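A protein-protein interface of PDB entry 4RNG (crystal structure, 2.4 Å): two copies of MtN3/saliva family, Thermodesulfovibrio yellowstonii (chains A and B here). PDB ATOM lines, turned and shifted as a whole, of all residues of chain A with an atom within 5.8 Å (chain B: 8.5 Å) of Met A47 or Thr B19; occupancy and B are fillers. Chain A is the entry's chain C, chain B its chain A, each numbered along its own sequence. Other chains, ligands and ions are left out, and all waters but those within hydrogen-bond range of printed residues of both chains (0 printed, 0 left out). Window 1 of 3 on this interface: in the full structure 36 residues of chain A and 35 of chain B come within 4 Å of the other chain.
Met B43 touches its own counterpart, Met A43. Phe A44 touches Met B43, but with the chains exchanged Met A43 does not touch Phe B44 (4.04 Å). Positions printed for both chains: 43, 44, 47, 51 and 77. Of the 19 pairs that touch across the chains among the printed residues, 1 has its exchanged pair printed and touching as well.
O of Ala B15 lies within hydrogen-bond range of NE1 of Trp A54 (3.4 Å). OG1 of Thr B19 lies within hydrogen-bond range of NE1 of Trp A54 (2.9 Å). The backbone carbonyl oxygen of Thr B19 lies close to the side-chain sulfur of Met A47 (3.5 Å).
Of the printed residues of chain B, Met A47 touches Thr B19 (3.5 Å) and Ala B22 (3.8 Å). Of chain A, only Met A47 (3.5 Å), Gly A50 (3.5 Å), Ile A51 (3.6 Å) and Trp A54 (2.9 Å) come within 4 Å of Thr B19. Printed residues of chain A within 4 Å of Pro B65: Trp A54 (3.9 Å). Printed residues of chain B within 4 Å of Met A43: Ala B22 (3.1 Å), Leu B23 (3.6 Å) and Met B43 (3.9 Å). Of the printed residues of chain B, Trp A54 touches Gly B12, Ala B15, Gly B16, Thr B19, Pro B65 and Ala B69. The nearest printed residue of chain B that does not touch Ala A42 is Ala B22 (5.0 Å).
Among the printed residues, merely in contact across the chains: Met A43 with Ala B22 (3.1 Å), Phe A46 with Ile B18 (3.2 Å), Trp A54 with Gly B16 (3.3 Å), Gly A50 with Ile B18 (3.4 Å), Gly A50 with Thr B19 (3.5 Å), Met A43 with Leu B23 (3.6 Å), Ile A51 with Thr B19 (3.6 Å), Trp A54 with Gly B12 (3.7 Å), Met A47 with Ala B22 (3.8 Å), Gly A50 with Ala B15 (3.8 Å), Met A43 with Met B43 (3.9 Å), Phe A46 with Ala B22 (3.9 Å), Ala A42 with Pro B25 (3.9 Å), Trp A54 with Pro B65 (3.9 Å), Trp A54 with Ala B69 (3.9 Å) and Phe A44 with Met B43 (3.97 Å).
Hydrophobic or aromatic side chains of chain B within 4 Å of the printed part of chain A: Ala B15, Ile B18, Ala B22, Leu B23, Pro B25, Met B43 and Ala B69. Hydrophobic or aromatic side chains of chain A that line the printed part of chain B: Ala A42, Met A43, Phe A44, Phe A46, Met A47 and Trp A54. Among the printed residues, 19 pairs touch across the chains. Among the printed residues, no Asp or Glu carboxylate lies within 4 Å of a Lys or Arg side-chain nitrogen of the other chain.
The side-chain hydroxyl of Thr B19 sits at hydrogen-bond distance from the backbone carbonyl oxygen of Ala B15 (3.2 Å). The backbone carbonyl oxygen (O) of Gly B16 sits at hydrogen-bond distance from the side-chain hydroxyl (OG1) of Thr B20, at 2.6 Å. The backbone carbonyl oxygen (O) of Ala B69 sits at hydrogen-bond distance from the side-chain hydroxyl (OG1) of Thr B20. O of Ala B69 sits at hydrogen-bond distance from OG of Ser B73 (2.6 Å).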
ATOM      1  N   ALA A  42     -19.394  29.491 -21.057  1.00  0.00           N
ATOM      2  CA  ALA A  42     -20.825  29.206 -20.926  1.00  0.00           C
ATOM      3  C   ALA A  42     -21.070  27.715 -20.922  1.00  0.00           C
ATOM      4  O   ALA A  42     -21.805  27.206 -20.078  1.00  0.00           O
ATOM      5  CB  ALA A  42     -21.622  29.872 -22.044  1.00  0.00           C
ATOM      6  N   MET A  43     -20.441  27.025 -21.864  1.00  0.00           N
ATOM      7  CA  MET A  43     -20.576  25.586 -21.985  1.00  0.00           C
ATOM      8  C   MET A  43     -20.258  24.891 -20.667  1.00  0.00           C
ATOM      9  O   MET A  43     -20.998  24.007 -20.232  1.00  0.00           O
ATOM     10  CB  MET A  43     -19.679  25.033 -23.104  1.00  0.00           C
ATOM     11  CG  MET A  43     -19.614  23.516 -23.081  1.00  0.00           C
ATOM     12  SD  MET A  43     -18.486  22.765 -24.252  1.00  0.00           S
ATOM     13  CE  MET A  43     -18.352  21.122 -23.545  1.00  0.00           C
ATOM     14  N   PHE A  44     -19.161  25.278 -20.029  1.00  0.00           N
ATOM     15  CA  PHE A  44     -18.774  24.572 -18.817  1.00  0.00           C
ATOM     16  C   PHE A  44     -19.609  25.014 -17.622  1.00  0.00           C
ATOM     17  O   PHE A  44     -19.893  24.203 -16.734  1.00  0.00           O
ATOM     18  CB  PHE A  44     -17.290  24.747 -18.541  1.00  0.00           C
ATOM     19  CG  PHE A  44     -16.427  23.885 -19.413  1.00  0.00           C
ATOM     20  CD1 PHE A  44     -16.313  22.531 -19.165  1.00  0.00           C
ATOM     21  CD2 PHE A  44     -15.767  24.420 -20.508  1.00  0.00           C
ATOM     22  CE1 PHE A  44     -15.543  21.733 -19.978  1.00  0.00           C
ATOM     23  CE2 PHE A  44     -14.989  23.626 -21.323  1.00  0.00           C
ATOM     24  CZ  PHE A  44     -14.877  22.278 -21.058  1.00  0.00           C
ATOM     25  N   ILE A  45     -20.038  26.274 -17.612  1.00  0.00           N
ATOM     26  CA  ILE A  45     -20.921  26.740 -16.554  1.00  0.00           C
ATOM     27  C   ILE A  45     -22.176  25.897 -16.506  1.00  0.00           C
ATOM     28  O   ILE A  45     -22.517  25.314 -15.486  1.00  0.00           O
ATOM     29  CB  ILE A  45     -21.353  28.195 -16.764  1.00  0.00           C
ATOM     30  CG1 ILE A  45     -20.207  29.172 -16.532  1.00  0.00           C
ATOM     31  CG2 ILE A  45     -22.451  28.558 -15.799  1.00  0.00           C
ATOM     32  CD1 ILE A  45     -20.647  30.621 -16.808  1.00  0.00           C
ATOM     33  N   PHE A  46     -22.853  25.825 -17.638  1.00  0.00           N
ATOM     34  CA  PHE A  46     -24.091  25.085 -17.723  1.00  0.00           C
ATOM     35  C   PHE A  46     -23.874  23.571 -17.661  1.00  0.00           C
ATOM     36  O   PHE A  46     -24.749  22.848 -17.201  1.00  0.00           O
ATOM     37  CB  PHE A  46     -24.841  25.517 -18.976  1.00  0.00           C
ATOM     38  CG  PHE A  46     -25.453  26.885 -18.843  1.00  0.00           C
ATOM     39  CD1 PHE A  46     -26.578  27.081 -18.066  1.00  0.00           C
ATOM     40  CD2 PHE A  46     -24.886  27.976 -19.470  1.00  0.00           C
ATOM     41  CE1 PHE A  46     -27.131  28.336 -17.923  1.00  0.00           C
ATOM     42  CE2 PHE A  46     -25.438  29.235 -19.334  1.00  0.00           C
ATOM     43  CZ  PHE A  46     -26.561  29.414 -18.559  1.00  0.00           C
ATOM     44  N   MET A  47     -22.735  23.089 -18.154  1.00  0.00           N
ATOM     45  CA  MET A  47     -22.423  21.672 -18.044  1.00  0.00           C
ATOM     46  C   MET A  47     -22.422  21.291 -16.560  1.00  0.00           C
ATOM     47  O   MET A  47     -23.030  20.294 -16.169  1.00  0.00           O
ATOM     48  CB  MET A  47     -21.057  21.326 -18.656  1.00  0.00           C
ATOM     49  CG  MET A  47     -21.091  20.787 -20.079  1.00  0.00           C
ATOM     50  SD  MET A  47     -22.354  19.528 -20.365  1.00  0.00           S
ATOM     51  CE  MET A  47     -21.738  18.184 -19.368  1.00  0.00           C
ATOM     52  N   ALA A  48     -21.763  22.111 -15.740  1.00  0.00           N
ATOM     53  CA  ALA A  48     -21.656  21.851 -14.310  1.00  0.00           C
ATOM     54  C   ALA A  48     -23.021  21.681 -13.649  1.00  0.00           C
ATOM     55  O   ALA A  48     -23.248  20.688 -12.948  1.00  0.00           O
ATOM     56  CB  ALA A  48     -20.881  22.961 -13.630  1.00  0.00           C
ATOM     57  N   ILE A  49     -23.936  22.626 -13.869  1.00  0.00           N
ATOM     58  CA  ILE A  49     -25.278  22.500 -13.282  1.00  0.00           C
ATOM     59  C   ILE A  49     -26.004  21.263 -13.776  1.00  0.00           C
ATOM     60  O   ILE A  49     -26.580  20.525 -12.969  1.00  0.00           O
ATOM     61  CB  ILE A  49     -26.164  23.706 -13.554  1.00  0.00           C
ATOM     62  CG1 ILE A  49     -25.579  24.941 -12.897  1.00  0.00           C
ATOM     63  CG2 ILE A  49     -27.543  23.478 -12.995  1.00  0.00           C
ATOM     64  CD1 ILE A  49     -25.068  25.860 -13.895  1.00  0.00           C
ATOM     65  N   GLY A  50     -25.976  21.038 -15.097  1.00  0.00           N
ATOM     66  CA  GLY A  50     -26.631  19.883 -15.676  1.00  0.00           C
ATOM     67  C   GLY A  50     -26.096  18.610 -15.065  1.00  0.00           C
ATOM     68  O   GLY A  50     -26.855  17.747 -14.637  1.00  0.00           O
ATOM     69  N   ILE A  51     -24.777  18.545 -14.952  1.00  0.00           N
ATOM     70  CA  ILE A  51     -24.087  17.403 -14.374  1.00  0.00           C
ATOM     71  C   ILE A  51     -24.458  17.186 -12.911  1.00  0.00           C
ATOM     72  O   ILE A  51     -24.604  16.044 -12.472  1.00  0.00           O
ATOM     73  CB  ILE A  51     -22.559  17.578 -14.498  1.00  0.00           C
ATOM     74  CG1 ILE A  51     -22.137  17.260 -15.923  1.00  0.00           C
ATOM     75  CG2 ILE A  51     -21.810  16.648 -13.548  1.00  0.00           C
ATOM     76  CD1 ILE A  51     -20.672  17.316 -16.123  1.00  0.00           C
ATOM     77  N   THR A  52     -24.654  18.273 -12.172  1.00  0.00           N
ATOM     78  CA  THR A  52     -25.151  18.158 -10.807  1.00  0.00           C
ATOM     79  C   THR A  52     -26.560  17.543 -10.792  1.00  0.00           C
ATOM     80  O   THR A  52     -26.890  16.748  -9.915  1.00  0.00           O
ATOM     81  CB  THR A  52     -25.165  19.514 -10.097  1.00  0.00           C
ATOM     82  OG1 THR A  52     -26.506  20.023 -10.116  1.00  0.00           O
ATOM     83  N   TRP A  54     -27.704  15.519 -13.224  1.00  0.00           N
ATOM     84  CA  TRP A  54     -27.496  14.124 -13.601  1.00  0.00           C
ATOM     85  C   TRP A  54     -27.111  13.296 -12.367  1.00  0.00           C
ATOM     86  O   TRP A  54     -27.516  12.149 -12.221  1.00  0.00           O
ATOM     87  CB  TRP A  54     -26.404  14.010 -14.658  1.00  0.00           C
ATOM     88  CG  TRP A  54     -26.882  14.246 -16.038  1.00  0.00           C
ATOM     89  CD1 TRP A  54     -26.480  15.237 -16.882  1.00  0.00           C
ATOM     90  CD2 TRP A  54     -27.854  13.483 -16.755  1.00  0.00           C
ATOM     91  NE1 TRP A  54     -27.138  15.135 -18.077  1.00  0.00           N
ATOM     92  CE2 TRP A  54     -28.004  14.056 -18.019  1.00  0.00           C
ATOM     93  CE3 TRP A  54     -28.627  12.354 -16.439  1.00  0.00           C
ATOM     94  CZ2 TRP A  54     -28.875  13.558 -18.986  1.00  0.00           C
ATOM     95  CZ3 TRP A  54     -29.501  11.860 -17.387  1.00  0.00           C
ATOM     96  CH2 TRP A  54     -29.617  12.461 -18.648  1.00  0.00           C
ATOM     97  N   ILE A  77     -14.484  19.567 -14.199  1.00  0.00           N
ATOM     98  CA  ILE A  77     -15.055  20.735 -14.861  1.00  0.00           C
ATOM     99  C   ILE A  77     -14.742  21.984 -14.080  1.00  0.00           C
ATOM    100  O   ILE A  77     -14.386  23.013 -14.655  1.00  0.00           O
ATOM    101  CB  ILE A  77     -16.559  20.599 -15.059  1.00  0.00           C
ATOM    102  CG1 ILE A  77     -16.813  19.824 -16.345  1.00  0.00           C
ATOM    103  CG2 ILE A  77     -17.218  21.953 -15.196  1.00  0.00           C
ATOM    104  CD1 ILE A  77     -18.272  19.622 -16.638  1.00  0.00           C
ATOM    105  N   GLY B  12     -34.223  13.827 -14.929  1.00  0.00           N
ATOM    106  CA  GLY B  12     -33.421  13.344 -16.031  1.00  0.00           C
ATOM    107  C   GLY B  12     -33.551  14.225 -17.249  1.00  0.00           C
ATOM    108  O   GLY B  12     -32.571  14.623 -17.866  1.00  0.00           O
ATOM    109  N   ILE B  13     -34.785  14.544 -17.582  1.00  0.00           N
ATOM    110  CA  ILE B  13     -35.049  15.329 -18.757  1.00  0.00           C
ATOM    111  C   ILE B  13     -34.457  16.700 -18.570  1.00  0.00           C
ATOM    112  O   ILE B  13     -33.800  17.219 -19.475  1.00  0.00           O
ATOM    113  CB  ILE B  13     -36.553  15.403 -19.030  1.00  0.00           C
ATOM    114  CG1 ILE B  13     -37.051  14.019 -19.459  1.00  0.00           C
ATOM    115  CG2 ILE B  13     -36.851  16.428 -20.083  1.00  0.00           C
ATOM    116  CD1 ILE B  13     -38.536  13.829 -19.345  1.00  0.00           C
ATOM    117  N   ILE B  14     -34.645  17.270 -17.381  1.00  0.00           N
ATOM    118  CA  ILE B  14     -34.127  18.610 -17.101  1.00  0.00           C
ATOM    119  C   ILE B  14     -32.594  18.576 -17.170  1.00  0.00           C
ATOM    120  O   ILE B  14     -31.991  19.440 -17.801  1.00  0.00           O
ATOM    121  CB  ILE B  14     -34.630  19.130 -15.733  1.00  0.00           C
ATOM    122  CG1 ILE B  14     -36.129  19.415 -15.823  1.00  0.00           C
ATOM    123  CG2 ILE B  14     -33.943  20.415 -15.334  1.00  0.00           C
ATOM    124  CD1 ILE B  14     -36.690  20.145 -14.639  1.00  0.00           C
ATOM    125  N   ALA B  15     -31.974  17.564 -16.558  1.00  0.00           N
ATOM    126  CA  ALA B  15     -30.534  17.381 -16.679  1.00  0.00           C
ATOM    127  C   ALA B  15     -30.096  17.257 -18.133  1.00  0.00           C
ATOM    128  O   ALA B  15     -29.127  17.895 -18.559  1.00  0.00           O
ATOM    129  CB  ALA B  15     -30.074  16.150 -15.901  1.00  0.00           C
ATOM    130  N   GLY B  16     -30.811  16.426 -18.885  1.00  0.00           N
ATOM    131  CA  GLY B  16     -30.454  16.156 -20.264  1.00  0.00           C
ATOM    132  C   GLY B  16     -30.609  17.380 -21.131  1.00  0.00           C
ATOM    133  O   GLY B  16     -29.791  17.619 -22.013  1.00  0.00           O
ATOM    134  N   ALA B  17     -31.651  18.166 -20.871  1.00  0.00           N
ATOM    135  CA  ALA B  17     -31.852  19.429 -21.571  1.00  0.00           C
ATOM    136  C   ALA B  17     -30.716  20.394 -21.247  1.00  0.00           C
ATOM    137  O   ALA B  17     -30.197  21.095 -22.138  1.00  0.00           O
ATOM    138  CB  ALA B  17     -33.192  20.038 -21.212  1.00  0.00           C
ATOM    139  N   ILE B  18     -30.310  20.428 -19.981  1.00  0.00           N
ATOM    140  CA  ILE B  18     -29.242  21.339 -19.642  1.00  0.00           C
ATOM    141  C   ILE B  18     -27.907  20.902 -20.256  1.00  0.00           C
ATOM    142  O   ILE B  18     -27.275  21.687 -20.954  1.00  0.00           O
ATOM    143  CB  ILE B  18     -29.087  21.487 -18.119  1.00  0.00           C
ATOM    144  CG1 ILE B  18     -30.321  22.169 -17.542  1.00  0.00           C
ATOM    145  CG2 ILE B  18     -27.849  22.318 -17.762  1.00  0.00           C
ATOM    146  CD1 ILE B  18     -30.214  22.384 -16.088  1.00  0.00           C
ATOM    147  N   THR B  19     -27.493  19.654 -20.068  1.00  0.00           N
ATOM    148  CA  THR B  19     -26.164  19.280 -20.544  1.00  0.00           C
ATOM    149  C   THR B  19     -26.095  19.219 -22.054  1.00  0.00           C
ATOM    150  O   THR B  19     -25.066  19.521 -22.642  1.00  0.00           O
ATOM    151  CB  THR B  19     -25.671  17.938 -19.967  1.00  0.00           C
ATOM    152  OG1 THR B  19     -26.588  16.886 -20.300  1.00  0.00           O
ATOM    153  CG2 THR B  19     -25.530  18.058 -18.463  1.00  0.00           C
ATOM    154  N   THR B  20     -27.182  18.819 -22.691  1.00  0.00           N
ATOM    155  CA  THR B  20     -27.162  18.752 -24.132  1.00  0.00           C
ATOM    156  C   THR B  20     -27.025  20.162 -24.715  1.00  0.00           C
ATOM    157  O   THR B  20     -26.180  20.392 -25.588  1.00  0.00           O
ATOM    158  CB  THR B  20     -28.413  18.062 -24.657  1.00  0.00           C
ATOM    159  OG1 THR B  20     -28.513  16.759 -24.069  1.00  0.00           O
ATOM    160  CG2 THR B  20     -28.380  17.965 -26.158  1.00  0.00           C
ATOM    161  N   SER B  21     -27.820  21.107 -24.205  1.00  0.00           N
ATOM    162  CA  SER B  21     -27.837  22.480 -24.731  1.00  0.00           C
ATOM    163  C   SER B  21     -26.551  23.220 -24.416  1.00  0.00           C
ATOM    164  O   SER B  21     -26.155  24.126 -25.140  1.00  0.00           O
ATOM    165  CB  SER B  21     -28.986  23.278 -24.108  1.00  0.00           C
ATOM    166  OG  SER B  21     -30.212  22.594 -24.211  1.00  0.00           O
ATOM    167  N   ALA B  22     -25.888  22.786 -23.347  1.00  0.00           N
ATOM    168  CA  ALA B  22     -24.632  23.362 -22.899  1.00  0.00           C
ATOM    169  C   ALA B  22     -23.531  23.225 -23.950  1.00  0.00           C
ATOM    170  O   ALA B  22     -22.592  24.014 -23.965  1.00  0.00           O
ATOM    171  CB  ALA B  22     -24.202  22.729 -21.591  1.00  0.00           C
ATOM    172  N   LEU B  23     -23.638  22.232 -24.825  1.00  0.00           N
ATOM    173  CA  LEU B  23     -22.647  22.077 -25.877  1.00  0.00           C
ATOM    174  C   LEU B  23     -22.765  23.156 -26.968  1.00  0.00           C
ATOM    175  O   LEU B  23     -21.785  23.505 -27.625  1.00  0.00           O
ATOM    176  CB  LEU B  23     -22.773  20.698 -26.500  1.00  0.00           C
ATOM    177  CG  LEU B  23     -22.408  19.560 -25.555  1.00  0.00           C
ATOM    178  CD1 LEU B  23     -22.984  18.260 -26.088  1.00  0.00           C
ATOM    179  CD2 LEU B  23     -20.905  19.462 -25.445  1.00  0.00           C
ATOM    180  N   ILE B  24     -23.961  23.709 -27.138  1.00  0.00           N
ATOM    181  CA  ILE B  24     -24.186  24.689 -28.196  1.00  0.00           C
ATOM    182  C   ILE B  24     -23.288  25.948 -28.136  1.00  0.00           C
ATOM    183  O   ILE B  24     -22.720  26.340 -29.161  1.00  0.00           O
ATOM    184  CB  ILE B  24     -25.675  25.104 -28.243  1.00  0.00           C
ATOM    185  CG1 ILE B  24     -26.476  23.982 -28.885  1.00  0.00           C
ATOM    186  CG2 ILE B  24     -25.870  26.315 -29.106  1.00  0.00           C
ATOM    187  CD1 ILE B  24     -27.952  24.159 -28.797  1.00  0.00           C
ATOM    188  N   PRO B  25     -23.139  26.580 -26.959  1.00  0.00           N
ATOM    189  CA  PRO B  25     -22.264  27.759 -26.962  1.00  0.00           C
ATOM    190  C   PRO B  25     -20.829  27.519 -27.457  1.00  0.00           C
ATOM    191  O   PRO B  25     -20.258  28.427 -28.035  1.00  0.00           O
ATOM    192  CB  PRO B  25     -22.254  28.186 -25.489  1.00  0.00           C
ATOM    193  CG  PRO B  25     -23.551  27.741 -24.973  1.00  0.00           C
ATOM    194  CD  PRO B  25     -23.853  26.440 -25.678  1.00  0.00           C
ATOM    195  N   MET B  43     -10.492  15.939 -26.289  1.00  0.00           N
ATOM    196  CA  MET B  43     -11.641  15.923 -25.369  1.00  0.00           C
ATOM    197  C   MET B  43     -12.940  15.549 -26.078  1.00  0.00           C
ATOM    198  O   MET B  43     -13.707  14.733 -25.569  1.00  0.00           O
ATOM    199  CB  MET B  43     -11.835  17.264 -24.645  1.00  0.00           C
ATOM    200  CG  MET B  43     -13.192  17.348 -23.904  1.00  0.00           C
ATOM    201  SD  MET B  43     -13.607  18.940 -23.127  1.00  0.00           S
ATOM    202  CE  MET B  43     -15.370  18.783 -22.866  1.00  0.00           C
ATOM    203  N   PHE B  44     -13.192  16.134 -27.247  1.00  0.00           N
ATOM    204  CA  PHE B  44     -14.472  15.897 -27.920  1.00  0.00           C
ATOM    205  C   PHE B  44     -14.532  14.555 -28.637  1.00  0.00           C
ATOM    206  O   PHE B  44     -15.583  13.910 -28.676  1.00  0.00           O
ATOM    207  CB  PHE B  44     -14.769  17.037 -28.877  1.00  0.00           C
ATOM    208  CG  PHE B  44     -15.202  18.252 -28.165  1.00  0.00           C
ATOM    209  CD1 PHE B  44     -16.462  18.318 -27.618  1.00  0.00           C
ATOM    210  CD2 PHE B  44     -14.323  19.299 -27.966  1.00  0.00           C
ATOM    211  CE1 PHE B  44     -16.858  19.410 -26.929  1.00  0.00           C
ATOM    212  CE2 PHE B  44     -14.705  20.408 -27.270  1.00  0.00           C
ATOM    213  CZ  PHE B  44     -15.982  20.467 -26.747  1.00  0.00           C
ATOM    214  N   MET B  47     -15.241  12.357 -25.815  1.00  0.00           N
ATOM    215  CA  MET B  47     -16.620  12.523 -25.368  1.00  0.00           C
ATOM    216  C   MET B  47     -17.586  11.781 -26.289  1.00  0.00           C
ATOM    217  O   MET B  47     -18.491  11.084 -25.811  1.00  0.00           O
ATOM    218  CB  MET B  47     -16.996  13.994 -25.270  1.00  0.00           C
ATOM    219  CG  MET B  47     -16.900  14.523 -23.859  1.00  0.00           C
ATOM    220  SD  MET B  47     -17.482  16.208 -23.767  1.00  0.00           S
ATOM    221  CE  MET B  47     -19.219  15.939 -24.060  1.00  0.00           C
ATOM    222  N   ILE B  51     -20.076   9.157 -24.829  1.00  0.00           N
ATOM    223  CA  ILE B  51     -21.500   9.457 -24.915  1.00  0.00           C
ATOM    224  C   ILE B  51     -22.225   8.402 -25.755  1.00  0.00           C
ATOM    225  O   ILE B  51     -23.369   8.026 -25.466  1.00  0.00           O
ATOM    226  CB  ILE B  51     -21.734  10.858 -25.500  1.00  0.00           C
ATOM    227  CG1 ILE B  51     -21.358  11.901 -24.456  1.00  0.00           C
ATOM    228  CG2 ILE B  51     -23.184  11.046 -25.931  1.00  0.00           C
ATOM    229  CD1 ILE B  51     -21.639  13.306 -24.879  1.00  0.00           C
ATOM    230  N   PRO B  65     -34.544   9.240 -20.816  1.00  0.00           N
ATOM    231  CA  PRO B  65     -33.759  10.478 -20.771  1.00  0.00           C
ATOM    232  C   PRO B  65     -32.279  10.272 -21.051  1.00  0.00           C
ATOM    233  O   PRO B  65     -31.674  11.135 -21.676  1.00  0.00           O
ATOM    234  CB  PRO B  65     -33.970  10.971 -19.341  1.00  0.00           C
ATOM    235  CG  PRO B  65     -35.313  10.490 -18.994  1.00  0.00           C
ATOM    236  CD  PRO B  65     -35.402   9.118 -19.625  1.00  0.00           C
ATOM    237  N   ALA B  69     -30.992  12.173 -24.531  1.00  0.00           N
ATOM    238  CA  ALA B  69     -30.023  13.242 -24.270  1.00  0.00           C
ATOM    239  C   ALA B  69     -28.694  12.956 -24.959  1.00  0.00           C
ATOM    240  O   ALA B  69     -28.065  13.854 -25.525  1.00  0.00           O
ATOM    241  CB  ALA B  69     -29.804  13.416 -22.801  1.00  0.00           C
ATOM    242  N   ASN B  70     -28.268  11.700 -24.927  1.00  0.00           N
ATOM    243  CA  ASN B  70     -26.974  11.370 -25.492  1.00  0.00           C
ATOM    244  C   ASN B  70     -26.991  11.298 -27.036  1.00  0.00           C
ATOM    245  O   ASN B  70     -26.013  11.668 -27.689  1.00  0.00           O
ATOM    246  CB  ASN B  70     -26.431  10.099 -24.835  1.00  0.00           C
ATOM    247  CG  ASN B  70     -25.948  10.367 -23.406  1.00  0.00           C
ATOM    248  OD1 ASN B  70     -24.873  10.929 -23.204  1.00  0.00           O
ATOM    249  ND2 ASN B  70     -26.755  10.003 -22.418  1.00  0.00           N
ATOM    250  N   ILE B  72     -28.812  13.320 -28.958  1.00  0.00           N
ATOM    251  CA  ILE B  72     -28.756  14.691 -29.450  1.00  0.00           C
ATOM    252  C   ILE B  72     -27.357  15.273 -29.219  1.00  0.00           C
ATOM    253  O   ILE B  72     -26.805  15.961 -30.082  1.00  0.00           O
ATOM    254  CB  ILE B  72     -29.809  15.596 -28.798  1.00  0.00           C
ATOM    255  CG1 ILE B  72     -31.215  15.096 -29.125  1.00  0.00           C
ATOM    256  CG2 ILE B  72     -29.683  17.012 -29.308  1.00  0.00           C
ATOM    257  CD1 ILE B  72     -32.303  15.762 -28.297  1.00  0.00           C
ATOM    258  N   SER B  73     -26.775  14.955 -28.070  1.00  0.00           N
ATOM    259  CA  SER B  73     -25.416  15.371 -27.736  1.00  0.00           C
ATOM    260  C   SER B  73     -24.382  14.916 -28.757  1.00  0.00           C
ATOM    261  O   SER B  73     -23.460  15.656 -29.072  1.00  0.00           O
ATOM    262  CB  SER B  73     -25.043  14.840 -26.351  1.00  0.00           C
ATOM    263  OG  SER B  73     -25.937  15.364 -25.373  1.00  0.00           O
ATOM    264  N   LEU B  76     -24.359  17.187 -31.731  1.00  0.00           N
ATOM    265  CA  LEU B  76     -23.734  18.459 -31.409  1.00  0.00           C
ATOM    266  C   LEU B  76     -22.224  18.332 -31.251  1.00  0.00           C
ATOM    267  O   LEU B  76     -21.499  19.274 -31.528  1.00  0.00           O
ATOM    268  CB  LEU B  76     -24.343  19.066 -30.155  1.00  0.00           C
ATOM    269  CG  LEU B  76     -25.786  19.530 -30.300  1.00  0.00           C
ATOM    270  CD1 LEU B  76     -26.316  20.043 -28.951  1.00  0.00           C
ATOM    271  CD2 LEU B  76     -25.835  20.612 -31.344  1.00  0.00           C
ATOM    272  N   ILE B  77     -21.757  17.193 -30.750  1.00  0.00           N
ATOM    273  CA  ILE B  77     -20.328  16.980 -30.618  1.00  0.00           C
ATOM    274  C   ILE B  77     -19.647  16.863 -31.989  1.00  0.00           C
ATOM    275  O   ILE B  77     -18.584  17.425 -32.202  1.00  0.00           O
ATOM    276  CB  ILE B  77     -20.050  15.757 -29.761  1.00  0.00           C
ATOM    277  CG1 ILE B  77     -20.217  16.140 -28.294  1.00  0.00           C
ATOM    278  CG2 ILE B  77     -18.645  15.247 -29.995  1.00  0.00           C
ATOM    279  CD1 ILE B  77     -20.012  15.010 -27.377  1.00  0.00           C
